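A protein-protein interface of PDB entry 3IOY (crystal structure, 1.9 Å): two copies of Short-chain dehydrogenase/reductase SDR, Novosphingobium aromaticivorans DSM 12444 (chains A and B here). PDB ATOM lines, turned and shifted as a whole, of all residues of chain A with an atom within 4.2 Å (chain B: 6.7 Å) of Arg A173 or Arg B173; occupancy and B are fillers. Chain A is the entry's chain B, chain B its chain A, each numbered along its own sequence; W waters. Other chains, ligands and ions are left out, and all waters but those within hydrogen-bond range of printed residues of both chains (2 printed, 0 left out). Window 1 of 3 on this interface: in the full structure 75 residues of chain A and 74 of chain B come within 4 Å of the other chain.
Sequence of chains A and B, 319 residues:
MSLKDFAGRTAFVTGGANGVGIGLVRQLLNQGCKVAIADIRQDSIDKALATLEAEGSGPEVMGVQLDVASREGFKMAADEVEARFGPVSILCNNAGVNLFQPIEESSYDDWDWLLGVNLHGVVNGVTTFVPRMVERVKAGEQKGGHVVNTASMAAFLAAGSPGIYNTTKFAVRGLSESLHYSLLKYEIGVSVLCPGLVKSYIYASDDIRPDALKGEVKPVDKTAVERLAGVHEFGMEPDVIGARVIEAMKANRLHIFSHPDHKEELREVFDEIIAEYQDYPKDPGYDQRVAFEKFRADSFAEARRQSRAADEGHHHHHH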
ATOM      1  N   ALA A 155       2.592   7.166 -36.113  1.00  0.00           N
ATOM      2  CA  ALA A 155       1.677   6.149 -35.503  1.00  0.00           C
ATOM      3  C   ALA A 155       2.448   4.971 -34.898  1.00  0.00           C
ATOM      4  O   ALA A 155       1.852   4.061 -34.261  1.00  0.00           O
ATOM      5  CB  ALA A 155       0.715   5.633 -36.581  1.00  0.00           C
ATOM      6  N   PHE A 156       3.769   4.970 -35.130  1.00  0.00           N
ATOM      7  CA  PHE A 156       4.668   3.936 -34.629  1.00  0.00           C
ATOM      8  C   PHE A 156       5.841   4.528 -33.823  1.00  0.00           C
ATOM      9  O   PHE A 156       6.231   3.985 -32.799  1.00  0.00           O
ATOM     10  CB  PHE A 156       5.233   3.102 -35.786  1.00  0.00           C
ATOM     11  CG  PHE A 156       4.219   2.154 -36.419  1.00  0.00           C
ATOM     12  CD1 PHE A 156       3.911   0.939 -35.811  1.00  0.00           C
ATOM     13  CD2 PHE A 156       3.564   2.499 -37.591  1.00  0.00           C
ATOM     14  CE1 PHE A 156       2.980   0.080 -36.394  1.00  0.00           C
ATOM     15  CE2 PHE A 156       2.636   1.626 -38.189  1.00  0.00           C
ATOM     16  CZ  PHE A 156       2.353   0.451 -37.595  1.00  0.00           C
ATOM     17  N   LYS A 169      -2.196  10.436 -34.311  1.00  0.00           N
ATOM     18  CA  LYS A 169      -1.870   9.418 -35.311  1.00  0.00           C
ATOM     19  C   LYS A 169      -1.943   7.961 -34.789  1.00  0.00           C
ATOM     20  O   LYS A 169      -2.407   7.062 -35.532  1.00  0.00           O
ATOM     21  CB  LYS A 169      -0.520   9.725 -35.959  1.00  0.00           C
ATOM     22  CG  LYS A 169      -0.553  11.036 -36.726  1.00  0.00           C
ATOM     23  CD  LYS A 169      -1.657  11.061 -37.784  1.00  0.00           C
ATOM     24  CE  LYS A 169      -1.782  12.433 -38.453  1.00  0.00           C
ATOM     25  NZ  LYS A 169      -2.533  12.345 -39.748  1.00  0.00           N
ATOM     26  N   PHE A 170      -1.479   7.736 -33.560  1.00  0.00           N
ATOM     27  CA  PHE A 170      -1.750   6.473 -32.840  1.00  0.00           C
ATOM     28  C   PHE A 170      -3.251   6.218 -32.836  1.00  0.00           C
ATOM     29  O   PHE A 170      -3.696   5.091 -33.086  1.00  0.00           O
ATOM     30  CB  PHE A 170      -1.223   6.496 -31.389  1.00  0.00           C
ATOM     31  CG  PHE A 170       0.192   5.989 -31.256  1.00  0.00           C
ATOM     32  CD1 PHE A 170       1.270   6.736 -31.751  1.00  0.00           C
ATOM     33  CD2 PHE A 170       0.437   4.761 -30.688  1.00  0.00           C
ATOM     34  CE1 PHE A 170       2.618   6.255 -31.618  1.00  0.00           C
ATOM     35  CE2 PHE A 170       1.767   4.262 -30.571  1.00  0.00           C
ATOM     36  CZ  PHE A 170       2.854   5.011 -31.056  1.00  0.00           C
ATOM     37  N   ALA A 171      -4.036   7.257 -32.535  1.00  0.00           N
ATOM     38  CA  ALA A 171      -5.512   7.050 -32.450  1.00  0.00           C
ATOM     39  C   ALA A 171      -6.046   6.628 -33.816  1.00  0.00           C
ATOM     40  O   ALA A 171      -6.818   5.704 -33.886  1.00  0.00           O
ATOM     41  CB  ALA A 171      -6.223   8.295 -31.963  1.00  0.00           C
ATOM     42  N   VAL A 172      -5.630   7.290 -34.896  1.00  0.00           N
ATOM     43  CA  VAL A 172      -6.113   6.903 -36.242  1.00  0.00           C
ATOM     44  C   VAL A 172      -5.684   5.489 -36.593  1.00  0.00           C
ATOM     45  O   VAL A 172      -6.454   4.710 -37.221  1.00  0.00           O
ATOM     46  CB  VAL A 172      -5.618   7.871 -37.338  1.00  0.00           C
ATOM     47  CG1 VAL A 172      -5.927   7.359 -38.743  1.00  0.00           C
ATOM     48  CG2 VAL A 172      -6.233   9.302 -37.126  1.00  0.00           C
ATOM     49  N   ARG A 173      -4.483   5.116 -36.182  1.00  0.00           N
ATOM     50  CA  ARG A 173      -4.044   3.768 -36.485  1.00  0.00           C
ATOM     51  C   ARG A 173      -4.930   2.757 -35.747  1.00  0.00           C
ATOM     52  O   ARG A 173      -5.328   1.736 -36.329  1.00  0.00           O
ATOM     53  CB  ARG A 173      -2.583   3.577 -36.084  1.00  0.00           C
ATOM     54  CG  ARG A 173      -2.323   2.116 -35.919  1.00  0.00           C
ATOM     55  CD  ARG A 173      -0.954   1.794 -36.349  1.00  0.00           C
ATOM     56  NE  ARG A 173      -0.027   1.959 -35.260  1.00  0.00           N
ATOM     57  CZ  ARG A 173       0.458   0.989 -34.495  1.00  0.00           C
ATOM     58  NH1 ARG A 173       1.356   1.283 -33.543  1.00  0.00           N
ATOM     59  NH2 ARG A 173       0.056  -0.250 -34.649  1.00  0.00           N
ATOM     60  N   GLY A 174      -5.224   3.037 -34.475  1.00  0.00           N
ATOM     61  CA  GLY A 174      -6.042   2.119 -33.632  1.00  0.00           C
ATOM     62  C   GLY A 174      -7.470   1.969 -34.167  1.00  0.00           C
ATOM     63  O   GLY A 174      -8.069   0.842 -34.194  1.00  0.00           O
ATOM     64  N   LEU A 175      -8.035   3.116 -34.521  1.00  0.00           N
ATOM     65  CA  LEU A 175      -9.289   3.182 -35.267  1.00  0.00           C
ATOM     66  C   LEU A 175      -9.270   2.361 -36.565  1.00  0.00           C
ATOM     67  O   LEU A 175     -10.172   1.537 -36.792  1.00  0.00           O
ATOM     68  CB  LEU A 175      -9.674   4.666 -35.517  1.00  0.00           C
ATOM     69  CG  LEU A 175     -11.070   5.057 -36.063  1.00  0.00           C
ATOM     70  CD1 LEU A 175     -11.271   6.601 -36.001  1.00  0.00           C
ATOM     71  CD2 LEU A 175     -11.272   4.595 -37.532  1.00  0.00           C
ATOM     72  N   SER A 176      -8.271   2.566 -37.411  1.00  0.00           N
ATOM     73  CA  SER A 176      -8.177   1.828 -38.685  1.00  0.00           C
ATOM     74  C   SER A 176      -8.047   0.326 -38.526  1.00  0.00           C
ATOM     75  O   SER A 176      -8.688  -0.415 -39.238  1.00  0.00           O
ATOM     76  CB  SER A 176      -7.021   2.374 -39.505  1.00  0.00           C
ATOM     77  OG  SER A 176      -7.197   3.764 -39.632  1.00  0.00           O
ATOM     78  N   GLU A 177      -7.220  -0.117 -37.559  1.00  0.00           N
ATOM     79  CA  GLU A 177      -7.005  -1.520 -37.322  1.00  0.00           C
ATOM     80  C   GLU A 177      -8.344  -2.146 -36.882  1.00  0.00           C
ATOM     81  O   GLU A 177      -8.738  -3.207 -37.433  1.00  0.00           O
ATOM     82  CB  GLU A 177      -5.878  -1.739 -36.271  1.00  0.00           C
ATOM     83  CG  GLU A 177      -4.480  -1.393 -36.839  1.00  0.00           C
ATOM     84  CD  GLU A 177      -3.329  -1.723 -35.857  1.00  0.00           C
ATOM     85  OE1 GLU A 177      -3.574  -2.402 -34.856  1.00  0.00           O
ATOM     86  OE2 GLU A 177      -2.195  -1.305 -36.110  1.00  0.00           O
ATOM     87  N   HIS A 255      -1.528  -2.154 -43.064  1.00  0.00           N
ATOM     88  CA  HIS A 255      -0.577  -1.043 -42.989  1.00  0.00           C
ATOM     89  C   HIS A 255       0.081  -0.815 -44.336  1.00  0.00           C
ATOM     90  O   HIS A 255       0.650  -1.740 -44.908  1.00  0.00           O
ATOM     91  CB  HIS A 255       0.501  -1.325 -41.919  1.00  0.00           C
ATOM     92  CG  HIS A 255      -0.072  -1.635 -40.579  1.00  0.00           C
ATOM     93  ND1 HIS A 255      -0.276  -2.917 -40.151  1.00  0.00           N
ATOM     94  CD2 HIS A 255      -0.570  -0.829 -39.609  1.00  0.00           C
ATOM     95  CE1 HIS A 255      -0.844  -2.899 -38.956  1.00  0.00           C
ATOM     96  NE2 HIS A 255      -1.053  -1.644 -38.615  1.00  0.00           N
ATOM     97  N   ILE A 273      10.365  -2.983 -27.330  1.00  0.00           N
ATOM     98  CA  ILE A 273       9.080  -3.218 -26.665  1.00  0.00           C
ATOM     99  C   ILE A 273       8.948  -4.614 -26.071  1.00  0.00           C
ATOM    100  O   ILE A 273       8.546  -4.733 -24.921  1.00  0.00           O
ATOM    101  CB  ILE A 273       7.847  -2.889 -27.579  1.00  0.00           C
ATOM    102  CG1 ILE A 273       7.844  -1.381 -27.900  1.00  0.00           C
ATOM    103  CG2 ILE A 273       6.538  -3.335 -26.868  1.00  0.00           C
ATOM    104  CD1 ILE A 273       6.869  -0.943 -29.013  1.00  0.00           C
ATOM    105  N   ASN B 149      -0.421   6.420 -16.905  1.00  0.00           N
ATOM    106  CA  ASN B 149      -1.712   6.465 -17.644  1.00  0.00           C
ATOM    107  C   ASN B 149      -2.141   5.033 -17.913  1.00  0.00           C
ATOM    108  O   ASN B 149      -1.348   4.223 -18.449  1.00  0.00           O
ATOM    109  CB  ASN B 149      -1.522   7.177 -18.979  1.00  0.00           C
ATOM    110  CG  ASN B 149      -1.121   8.633 -18.817  1.00  0.00           C
ATOM    111  OD1 ASN B 149      -1.587   9.312 -17.904  1.00  0.00           O
ATOM    112  ND2 ASN B 149      -0.295   9.132 -19.722  1.00  0.00           N
ATOM    113  N   ALA B 151      -3.590   2.556 -20.016  1.00  0.00           N
ATOM    114  CA  ALA B 151      -4.148   2.129 -21.286  1.00  0.00           C
ATOM    115  C   ALA B 151      -4.647   0.671 -21.142  1.00  0.00           C
ATOM    116  O   ALA B 151      -5.467   0.403 -20.283  1.00  0.00           O
ATOM    117  CB  ALA B 151      -3.183   2.344 -22.429  1.00  0.00           C
ATOM    118  N   SER B 152      -4.137  -0.275 -21.916  1.00  0.00           N
ATOM    119  CA  SER B 152      -4.712  -1.619 -21.991  1.00  0.00           C
ATOM    120  C   SER B 152      -3.841  -2.389 -22.992  1.00  0.00           C
ATOM    121  O   SER B 152      -3.165  -1.758 -23.778  1.00  0.00           O
ATOM    122  CB  SER B 152      -6.140  -1.487 -22.587  1.00  0.00           C
ATOM    123  OG  SER B 152      -6.651  -2.745 -22.973  1.00  0.00           O
ATOM    124  N   ALA B 155      -4.119  -1.265 -26.497  1.00  0.00           N
ATOM    125  CA  ALA B 155      -3.224  -0.298 -27.155  1.00  0.00           C
ATOM    126  C   ALA B 155      -2.209  -0.930 -28.126  1.00  0.00           C
ATOM    127  O   ALA B 155      -1.445  -0.234 -28.774  1.00  0.00           O
ATOM    128  CB  ALA B 155      -2.514   0.658 -26.100  1.00  0.00           C
ATOM    129  N   PHE B 156      -2.228  -2.255 -28.234  1.00  0.00           N
ATOM    130  CA  PHE B 156      -1.398  -3.004 -29.159  1.00  0.00           C
ATOM    131  C   PHE B 156      -2.212  -3.982 -29.985  1.00  0.00           C
ATOM    132  O   PHE B 156      -1.913  -4.219 -31.153  1.00  0.00           O
ATOM    133  CB  PHE B 156      -0.354  -3.832 -28.382  1.00  0.00           C
ATOM    134  CG  PHE B 156       0.715  -2.996 -27.715  1.00  0.00           C
ATOM    135  CD1 PHE B 156       1.828  -2.576 -28.452  1.00  0.00           C
ATOM    136  CD2 PHE B 156       0.583  -2.608 -26.382  1.00  0.00           C
ATOM    137  CE1 PHE B 156       2.817  -1.803 -27.845  1.00  0.00           C
ATOM    138  CE2 PHE B 156       1.579  -1.833 -25.747  1.00  0.00           C
ATOM    139  CZ  PHE B 156       2.701  -1.430 -26.498  1.00  0.00           C
ATOM    140  N   LEU B 157      -3.209  -4.585 -29.359  1.00  0.00           N
ATOM    141  CA  LEU B 157      -3.894  -5.723 -29.988  1.00  0.00           C
ATOM    142  C   LEU B 157      -5.314  -5.238 -30.266  1.00  0.00           C
ATOM    143  O   LEU B 157      -6.120  -5.193 -29.345  1.00  0.00           O
ATOM    144  CB  LEU B 157      -3.883  -6.953 -29.054  1.00  0.00           C
ATOM    145  CG  LEU B 157      -2.447  -7.447 -28.764  1.00  0.00           C
ATOM    146  CD1 LEU B 157      -2.487  -8.546 -27.747  1.00  0.00           C
ATOM    147  CD2 LEU B 157      -1.662  -7.844 -30.038  1.00  0.00           C
ATOM    148  N   ALA B 158      -5.578  -4.800 -31.492  1.00  0.00           N
ATOM    149  CA  ALA B 158      -6.893  -4.184 -31.810  1.00  0.00           C
ATOM    150  C   ALA B 158      -7.656  -5.101 -32.752  1.00  0.00           C
ATOM    151  O   ALA B 158      -7.254  -5.283 -33.907  1.00  0.00           O
ATOM    152  CB  ALA B 158      -6.732  -2.782 -32.449  1.00  0.00           C
ATOM    153  N   THR B 167      -9.386   2.578 -30.048  1.00  0.00           N
ATOM    154  CA  THR B 167      -8.937   3.903 -30.535  1.00  0.00           C
ATOM    155  C   THR B 167      -8.403   4.783 -29.390  1.00  0.00           C
ATOM    156  O   THR B 167      -7.321   5.386 -29.520  1.00  0.00           O
ATOM    157  CB  THR B 167     -10.052   4.685 -31.314  1.00  0.00           C
ATOM    158  OG1 THR B 167     -10.520   3.868 -32.390  1.00  0.00           O
ATOM    159  CG2 THR B 167      -9.516   6.023 -31.878  1.00  0.00           C
ATOM    160  N   THR B 168      -9.165   4.876 -28.292  1.00  0.00           N
ATOM    161  CA  THR B 168      -8.761   5.732 -27.179  1.00  0.00           C
ATOM    162  C   THR B 168      -7.513   5.171 -26.442  1.00  0.00           C
ATOM    163  O   THR B 168      -6.705   5.936 -25.918  1.00  0.00           O
ATOM    164  CB  THR B 168      -9.874   5.882 -26.161  1.00  0.00           C
ATOM    165  OG1 THR B 168     -10.101   4.626 -25.504  1.00  0.00           O
ATOM    166  CG2 THR B 168     -11.182   6.412 -26.829  1.00  0.00           C
ATOM    167  N   LYS B 169      -7.359   3.850 -26.425  1.00  0.00           N
ATOM    168  CA  LYS B 169      -6.199   3.238 -25.776  1.00  0.00           C
ATOM    169  C   LYS B 169      -4.919   3.383 -26.593  1.00  0.00           C
ATOM    170  O   LYS B 169      -3.857   3.647 -26.007  1.00  0.00           O
ATOM    171  CB  LYS B 169      -6.472   1.789 -25.378  1.00  0.00           C
ATOM    172  CG  LYS B 169      -7.553   1.685 -24.309  1.00  0.00           C
ATOM    173  CD  LYS B 169      -7.254   2.571 -23.088  1.00  0.00           C
ATOM    174  CE  LYS B 169      -8.473   2.626 -22.180  1.00  0.00           C
ATOM    175  NZ  LYS B 169      -8.098   2.881 -20.760  1.00  0.00           N
ATOM    176  N   PHE B 170      -5.015   3.281 -27.919  1.00  0.00           N
ATOM    177  CA  PHE B 170      -3.876   3.567 -28.808  1.00  0.00           C
ATOM    178  C   PHE B 170      -3.490   5.038 -28.609  1.00  0.00           C
ATOM    179  O   PHE B 170      -2.334   5.382 -28.519  1.00  0.00           O
ATOM    180  CB  PHE B 170      -4.258   3.375 -30.272  1.00  0.00           C
ATOM    181  CG  PHE B 170      -3.849   2.020 -30.855  1.00  0.00           C
ATOM    182  CD1 PHE B 170      -4.510   0.870 -30.491  1.00  0.00           C
ATOM    183  CD2 PHE B 170      -2.812   1.942 -31.768  1.00  0.00           C
ATOM    184  CE1 PHE B 170      -4.131  -0.353 -31.008  1.00  0.00           C
ATOM    185  CE2 PHE B 170      -2.413   0.710 -32.293  1.00  0.00           C
ATOM    186  CZ  PHE B 170      -3.075  -0.440 -31.888  1.00  0.00           C
ATOM    187  N   ALA B 171      -4.483   5.913 -28.550  1.00  0.00           N
ATOM    188  CA  ALA B 171      -4.201   7.339 -28.356  1.00  0.00           C
ATOM    189  C   ALA B 171      -3.468   7.601 -27.038  1.00  0.00           C
ATOM    190  O   ALA B 171      -2.522   8.357 -27.025  1.00  0.00           O
ATOM    191  CB  ALA B 171      -5.524   8.169 -28.416  1.00  0.00           C
ATOM    192  N   VAL B 172      -3.925   7.009 -25.939  1.00  0.00           N
ATOM    193  CA  VAL B 172      -3.275   7.129 -24.621  1.00  0.00           C
ATOM    194  C   VAL B 172      -1.816   6.613 -24.693  1.00  0.00           C
ATOM    195  O   VAL B 172      -0.905   7.223 -24.125  1.00  0.00           O
ATOM    196  CB  VAL B 172      -4.103   6.431 -23.506  1.00  0.00           C
ATOM    197  CG1 VAL B 172      -3.341   6.351 -22.171  1.00  0.00           C
ATOM    198  CG2 VAL B 172      -5.420   7.193 -23.277  1.00  0.00           C
ATOM    199  N   ARG B 173      -1.578   5.531 -25.433  1.00  0.00           N
ATOM    200  CA  ARG B 173      -0.219   5.049 -25.625  1.00  0.00           C
ATOM    201  C   ARG B 173       0.644   6.103 -26.361  1.00  0.00           C
ATOM    202  O   ARG B 173       1.748   6.393 -25.908  1.00  0.00           O
ATOM    203  CB  ARG B 173      -0.238   3.683 -26.365  1.00  0.00           C
ATOM    204  CG  ARG B 173       1.167   3.085 -26.640  1.00  0.00           C
ATOM    205  CD  ARG B 173       1.032   1.811 -27.507  1.00  0.00           C
ATOM    206  NE  ARG B 173       2.242   1.628 -28.298  1.00  0.00           N
ATOM    207  CZ  ARG B 173       2.306   0.907 -29.399  1.00  0.00           C
ATOM    208  NH1 ARG B 173       1.223   0.270 -29.867  1.00  0.00           N
ATOM    209  NH2 ARG B 173       3.472   0.800 -30.018  1.00  0.00           N
ATOM    210  N   GLY B 174       0.143   6.677 -27.453  1.00  0.00           N
ATOM    211  CA  GLY B 174       0.924   7.650 -28.228  1.00  0.00           C
ATOM    212  C   GLY B 174       1.206   8.895 -27.382  1.00  0.00           C
ATOM    213  O   GLY B 174       2.301   9.518 -27.495  1.00  0.00           O
ATOM    214  N   LEU B 175       0.190   9.320 -26.633  1.00  0.00           N
ATOM    215  CA  LEU B 175       0.350  10.453 -25.697  1.00  0.00           C
ATOM    216  C   LEU B 175       1.457  10.137 -24.672  1.00  0.00           C
ATOM    217  O   LEU B 175       2.384  10.956 -24.445  1.00  0.00           O
ATOM    218  CB  LEU B 175      -0.989  10.795 -25.017  1.00  0.00           C
ATOM    219  CG  LEU B 175      -1.178  12.068 -24.177  1.00  0.00           C
ATOM    220  CD1 LEU B 175      -2.681  12.305 -24.044  1.00  0.00           C
ATOM    221  CD2 LEU B 175      -0.533  11.898 -22.764  1.00  0.00           C
ATOM    222  N   SER B 176       1.345   8.971 -24.043  1.00  0.00           N
ATOM    223  CA  SER B 176       2.236   8.591 -22.936  1.00  0.00           C
ATOM    224  C   SER B 176       3.682   8.438 -23.409  1.00  0.00           C
ATOM    225  O   SER B 176       4.634   8.788 -22.665  1.00  0.00           O
ATOM    226  CB  SER B 176       1.797   7.260 -22.337  1.00  0.00           C
ATOM    227  OG  SER B 176       0.478   7.382 -21.822  1.00  0.00           O
ATOM    228  N   GLU B 177       3.852   7.880 -24.615  1.00  0.00           N
ATOM    229  CA  GLU B 177       5.209   7.646 -25.148  1.00  0.00           C
ATOM    230  C   GLU B 177       5.818   9.021 -25.442  1.00  0.00           C
ATOM    231  O   GLU B 177       6.975   9.278 -25.061  1.00  0.00           O
ATOM    232  CB  GLU B 177       5.218   6.791 -26.420  1.00  0.00           C
ATOM    233  CG  GLU B 177       4.777   5.341 -26.165  1.00  0.00           C
ATOM    234  CD  GLU B 177       4.808   4.458 -27.442  1.00  0.00           C
ATOM    235  OE1 GLU B 177       5.218   4.937 -28.539  1.00  0.00           O
ATOM    236  OE2 GLU B 177       4.411   3.277 -27.329  1.00  0.00           O
ATOM    237  N   SER B 178       5.031   9.889 -26.079  1.00  0.00           N
ATOM    238  CA  SER B 178       5.507  11.254 -26.388  1.00  0.00           C
ATOM    239  C   SER B 178       5.909  12.019 -25.111  1.00  0.00           C
ATOM    240  O   SER B 178       7.015  12.566 -25.034  1.00  0.00           O
ATOM    241  CB  SER B 178       4.447  12.037 -27.165  1.00  0.00           C
ATOM    242  OG  SER B 178       4.132  11.349 -28.344  1.00  0.00           O
ATOM    243  N   VAL B 192       2.998   3.924 -19.265  1.00  0.00           N
ATOM    244  CA  VAL B 192       1.653   3.536 -19.706  1.00  0.00           C
ATOM    245  C   VAL B 192       1.441   2.092 -19.305  1.00  0.00           C
ATOM    246  O   VAL B 192       2.209   1.191 -19.705  1.00  0.00           O
ATOM    247  CB  VAL B 192       1.412   3.803 -21.225  1.00  0.00           C
ATOM    248  CG1 VAL B 192       2.448   3.108 -22.110  1.00  0.00           C
ATOM    249  CG2 VAL B 192      -0.031   3.395 -21.613  1.00  0.00           C
ATOM    250  N   CYS B 194      -0.381  -1.298 -19.312  1.00  0.00           N
ATOM    251  CA  CYS B 194      -1.095  -2.049 -20.356  1.00  0.00           C
ATOM    252  C   CYS B 194      -1.541  -3.418 -19.875  1.00  0.00           C
ATOM    253  O   CYS B 194      -1.002  -4.434 -20.331  1.00  0.00           O
ATOM    254  CB  CYS B 194      -0.229  -2.204 -21.581  1.00  0.00           C
ATOM    255  SG  CYS B 194       0.194  -0.580 -22.331  1.00  0.00           S
ATOM    256  N   LEU B 254       8.805   2.680 -19.618  1.00  0.00           N
ATOM    257  CA  LEU B 254       7.777   3.251 -20.507  1.00  0.00           C
ATOM    258  C   LEU B 254       6.486   2.377 -20.549  1.00  0.00           C
ATOM    259  O   LEU B 254       5.393   2.828 -20.157  1.00  0.00           O
ATOM    260  CB  LEU B 254       8.368   3.520 -21.892  1.00  0.00           C
ATOM    261  CG  LEU B 254       7.419   4.079 -22.972  1.00  0.00           C
ATOM    262  CD1 LEU B 254       6.578   5.255 -22.431  1.00  0.00           C
ATOM    263  CD2 LEU B 254       8.130   4.497 -24.238  1.00  0.00           C
ATOM    264  N   HIS B 255       6.627   1.121 -20.971  1.00  0.00           N
ATOM    265  CA  HIS B 255       5.504   0.198 -21.068  1.00  0.00           C
ATOM    266  C   HIS B 255       5.492  -0.728 -19.880  1.00  0.00           C
ATOM    267  O   HIS B 255       6.452  -1.479 -19.664  1.00  0.00           O
ATOM    268  CB  HIS B 255       5.585  -0.601 -22.408  1.00  0.00           C
ATOM    269  CG  HIS B 255       5.617   0.269 -23.633  1.00  0.00           C
ATOM    270  ND1 HIS B 255       6.776   0.534 -24.329  1.00  0.00           N
ATOM    271  CD2 HIS B 255       4.633   0.966 -24.267  1.00  0.00           C
ATOM    272  CE1 HIS B 255       6.509   1.339 -25.347  1.00  0.00           C
ATOM    273  NE2 HIS B 255       5.216   1.619 -25.328  1.00  0.00           N
ATOM    274  N   PHE B 270       4.018  -8.194 -34.110  1.00  0.00           N
ATOM    275  CA  PHE B 270       5.128  -7.347 -34.594  1.00  0.00           C
ATOM    276  C   PHE B 270       5.783  -7.915 -35.848  1.00  0.00           C
ATOM    277  O   PHE B 270       6.145  -7.164 -36.800  1.00  0.00           O
ATOM    278  CB  PHE B 270       6.209  -7.125 -33.482  1.00  0.00           C
ATOM    279  CG  PHE B 270       5.795  -6.147 -32.362  1.00  0.00           C
ATOM    280  CD1 PHE B 270       4.680  -5.303 -32.487  1.00  0.00           C
ATOM    281  CD2 PHE B 270       6.530  -6.088 -31.179  1.00  0.00           C
ATOM    282  CE1 PHE B 270       4.316  -4.405 -31.433  1.00  0.00           C
ATOM    283  CE2 PHE B 270       6.182  -5.195 -30.142  1.00  0.00           C
ATOM    284  CZ  PHE B 270       5.086  -4.356 -30.264  1.00  0.00           C
ATOM    285  N   ILE B 273       3.542  -7.152 -38.879  1.00  0.00           N
ATOM    286  CA  ILE B 273       3.715  -5.744 -39.358  1.00  0.00           C
ATOM    287  C   ILE B 273       4.992  -5.571 -40.166  1.00  0.00           C
ATOM    288  O   ILE B 273       5.005  -4.910 -41.224  1.00  0.00           O
ATOM    289  CB  ILE B 273       3.703  -4.737 -38.167  1.00  0.00           C
ATOM    290  CG1 ILE B 273       2.332  -4.762 -37.476  1.00  0.00           C
ATOM    291  CG2 ILE B 273       4.062  -3.310 -38.647  1.00  0.00           C
ATOM    292  CD1 ILE B 273       2.279  -3.915 -36.198  1.00  0.00           C
HETATM  293  O   HOH W   1       5.994   2.674 -29.984  1.00  0.00           O
HETATM  294  O   HOH W   2       2.933  -0.998 -32.223  1.00  0.00           O
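The side-chain hydroxyl (OG1) of Thr B167 sits close to the backbone NH (N) of Leu A175 (3.4 Å).
Water W1 lies within hydrogen-bond range of the side-chain carboxylate of Glu B177 (2.8 Å), the backbone carbonyl oxygen of Phe A156 (3.1 Å) and the guanidinium group of Arg B173 (3.1 Å). Water W2 bridges NH2 of Arg B173 and NH1 of Arg A173.
Arg A173 touches just these residues of chain B: Phe B170 and Arg B173. Arg B173 touches just these residues of chain A: Phe A170 (3.5 Å), Arg A173 (3.8 Å) and Ile A273 (3.9 Å). Of the printed residues of chain B, His A255 touches Ile B273 (3.97 Å). Printed residues of chain B within 4 Å of Phe A170: Phe B170 (3.3 Å), Arg B173 (3.5 Å), Gly B174 (3.5 Å) and Glu B177 (3.5 Å). Printed residues of chain B within 4 Å of Leu A175: Thr B167 (3.2 Å). Of the printed residues of chain A, Phe B270 touches Ile A273. Val B172 touches none of the printed residues of chain A. Ala B155 touches none of the printed residues of chain A. The nearest residue of chain B that does not touch Arg A173 is Ile B273 (4.6 Å). The nearest printed residue of chain B that does not touch His A255 is Phe B170 (6.9 Å).
Phe A170 touches Arg B173, and with the chains exchanged Arg A173 touches Phe B170. Phe A170 touches Gly B174, and with the chains exchanged Gly A174 touches Phe B170. Phe A170 touches Glu B177, and with the chains exchanged Glu A177 touches Phe B170. Arg A173 touches its own counterpart, Arg B173. Positions printed for both chains: 155, 156, 169, 170, 171, 172, 173, 174, 175, 176, 177, 255 and 273.
The side-chain carboxylate (OE2) of Glu B177 is in salt-bridge range of the guanidinium group (NE) of Arg B173 (2.9 Å). The guanidinium group (NH1) of Arg B173 lies within hydrogen-bond range of the backbone carbonyl oxygen (O) of Ala B155 (2.9 Å). The guanidinium group (NH2) of Arg A173 lies within salt-bridge range of the side-chain carboxylate (OE2) of Glu A177, at 2.9 Å. A ring nitrogen (NE2) of His B255 lies within hydrogen-bond range of the side-chain carboxylate of Glu B177. The side-chain carboxylate of Glu A177 sits at hydrogen-bond distance from a ring nitrogen (NE2) of His A255, 2.8 Å away. The backbone carbonyl oxygen (O) of Ala A155 lies within hydrogen-bond range of the guanidinium group (NH1) of Arg A173.
Phe A170 touches Phe B170 (CB to O, 3.3 Å). Arg B173 touches Phe A170. Ala A171 touches Thr B167 (O to CG2, 3.4 Å). Arg A173 touches Phe B170 (NH2 to CE2, 3.5 Å). Phe B170 touches Gly A174 (CG to CA, 3.5 Å). Glu A177 touches Ala B158. Phe B170 touches Glu A177 (CZ to OE1, 3.6 Å). CE1 of His A255 touches CG1 of Ile B273, 3.97 Å away. His B255 touches Ile A273. Ile A273 touches Phe B270 (CG2 to CE2, 3.8 Å).
Hydrophobic or aromatic side chains of chain B that line the printed part of chain A: Ala B158, Phe B170, Ala B171, His B255, Phe B270 and Ile B273. Printed residues of chain A that touch a printed residue of chain B: Phe A170, Ala A171, Arg A173, Gly A174, Leu A175, Glu A177, His A255 and Ile A273. Hydrophobic or aromatic side chains of chain A within 4 Å of the printed part of chain B: Phe A170, Ala A171, Leu A175, His A255 and Ile A273. Along chain A the printed residues that touch a printed residue of chain B span positions 170 to 273. Among the printed residues, 16 pairs touch across the chains.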
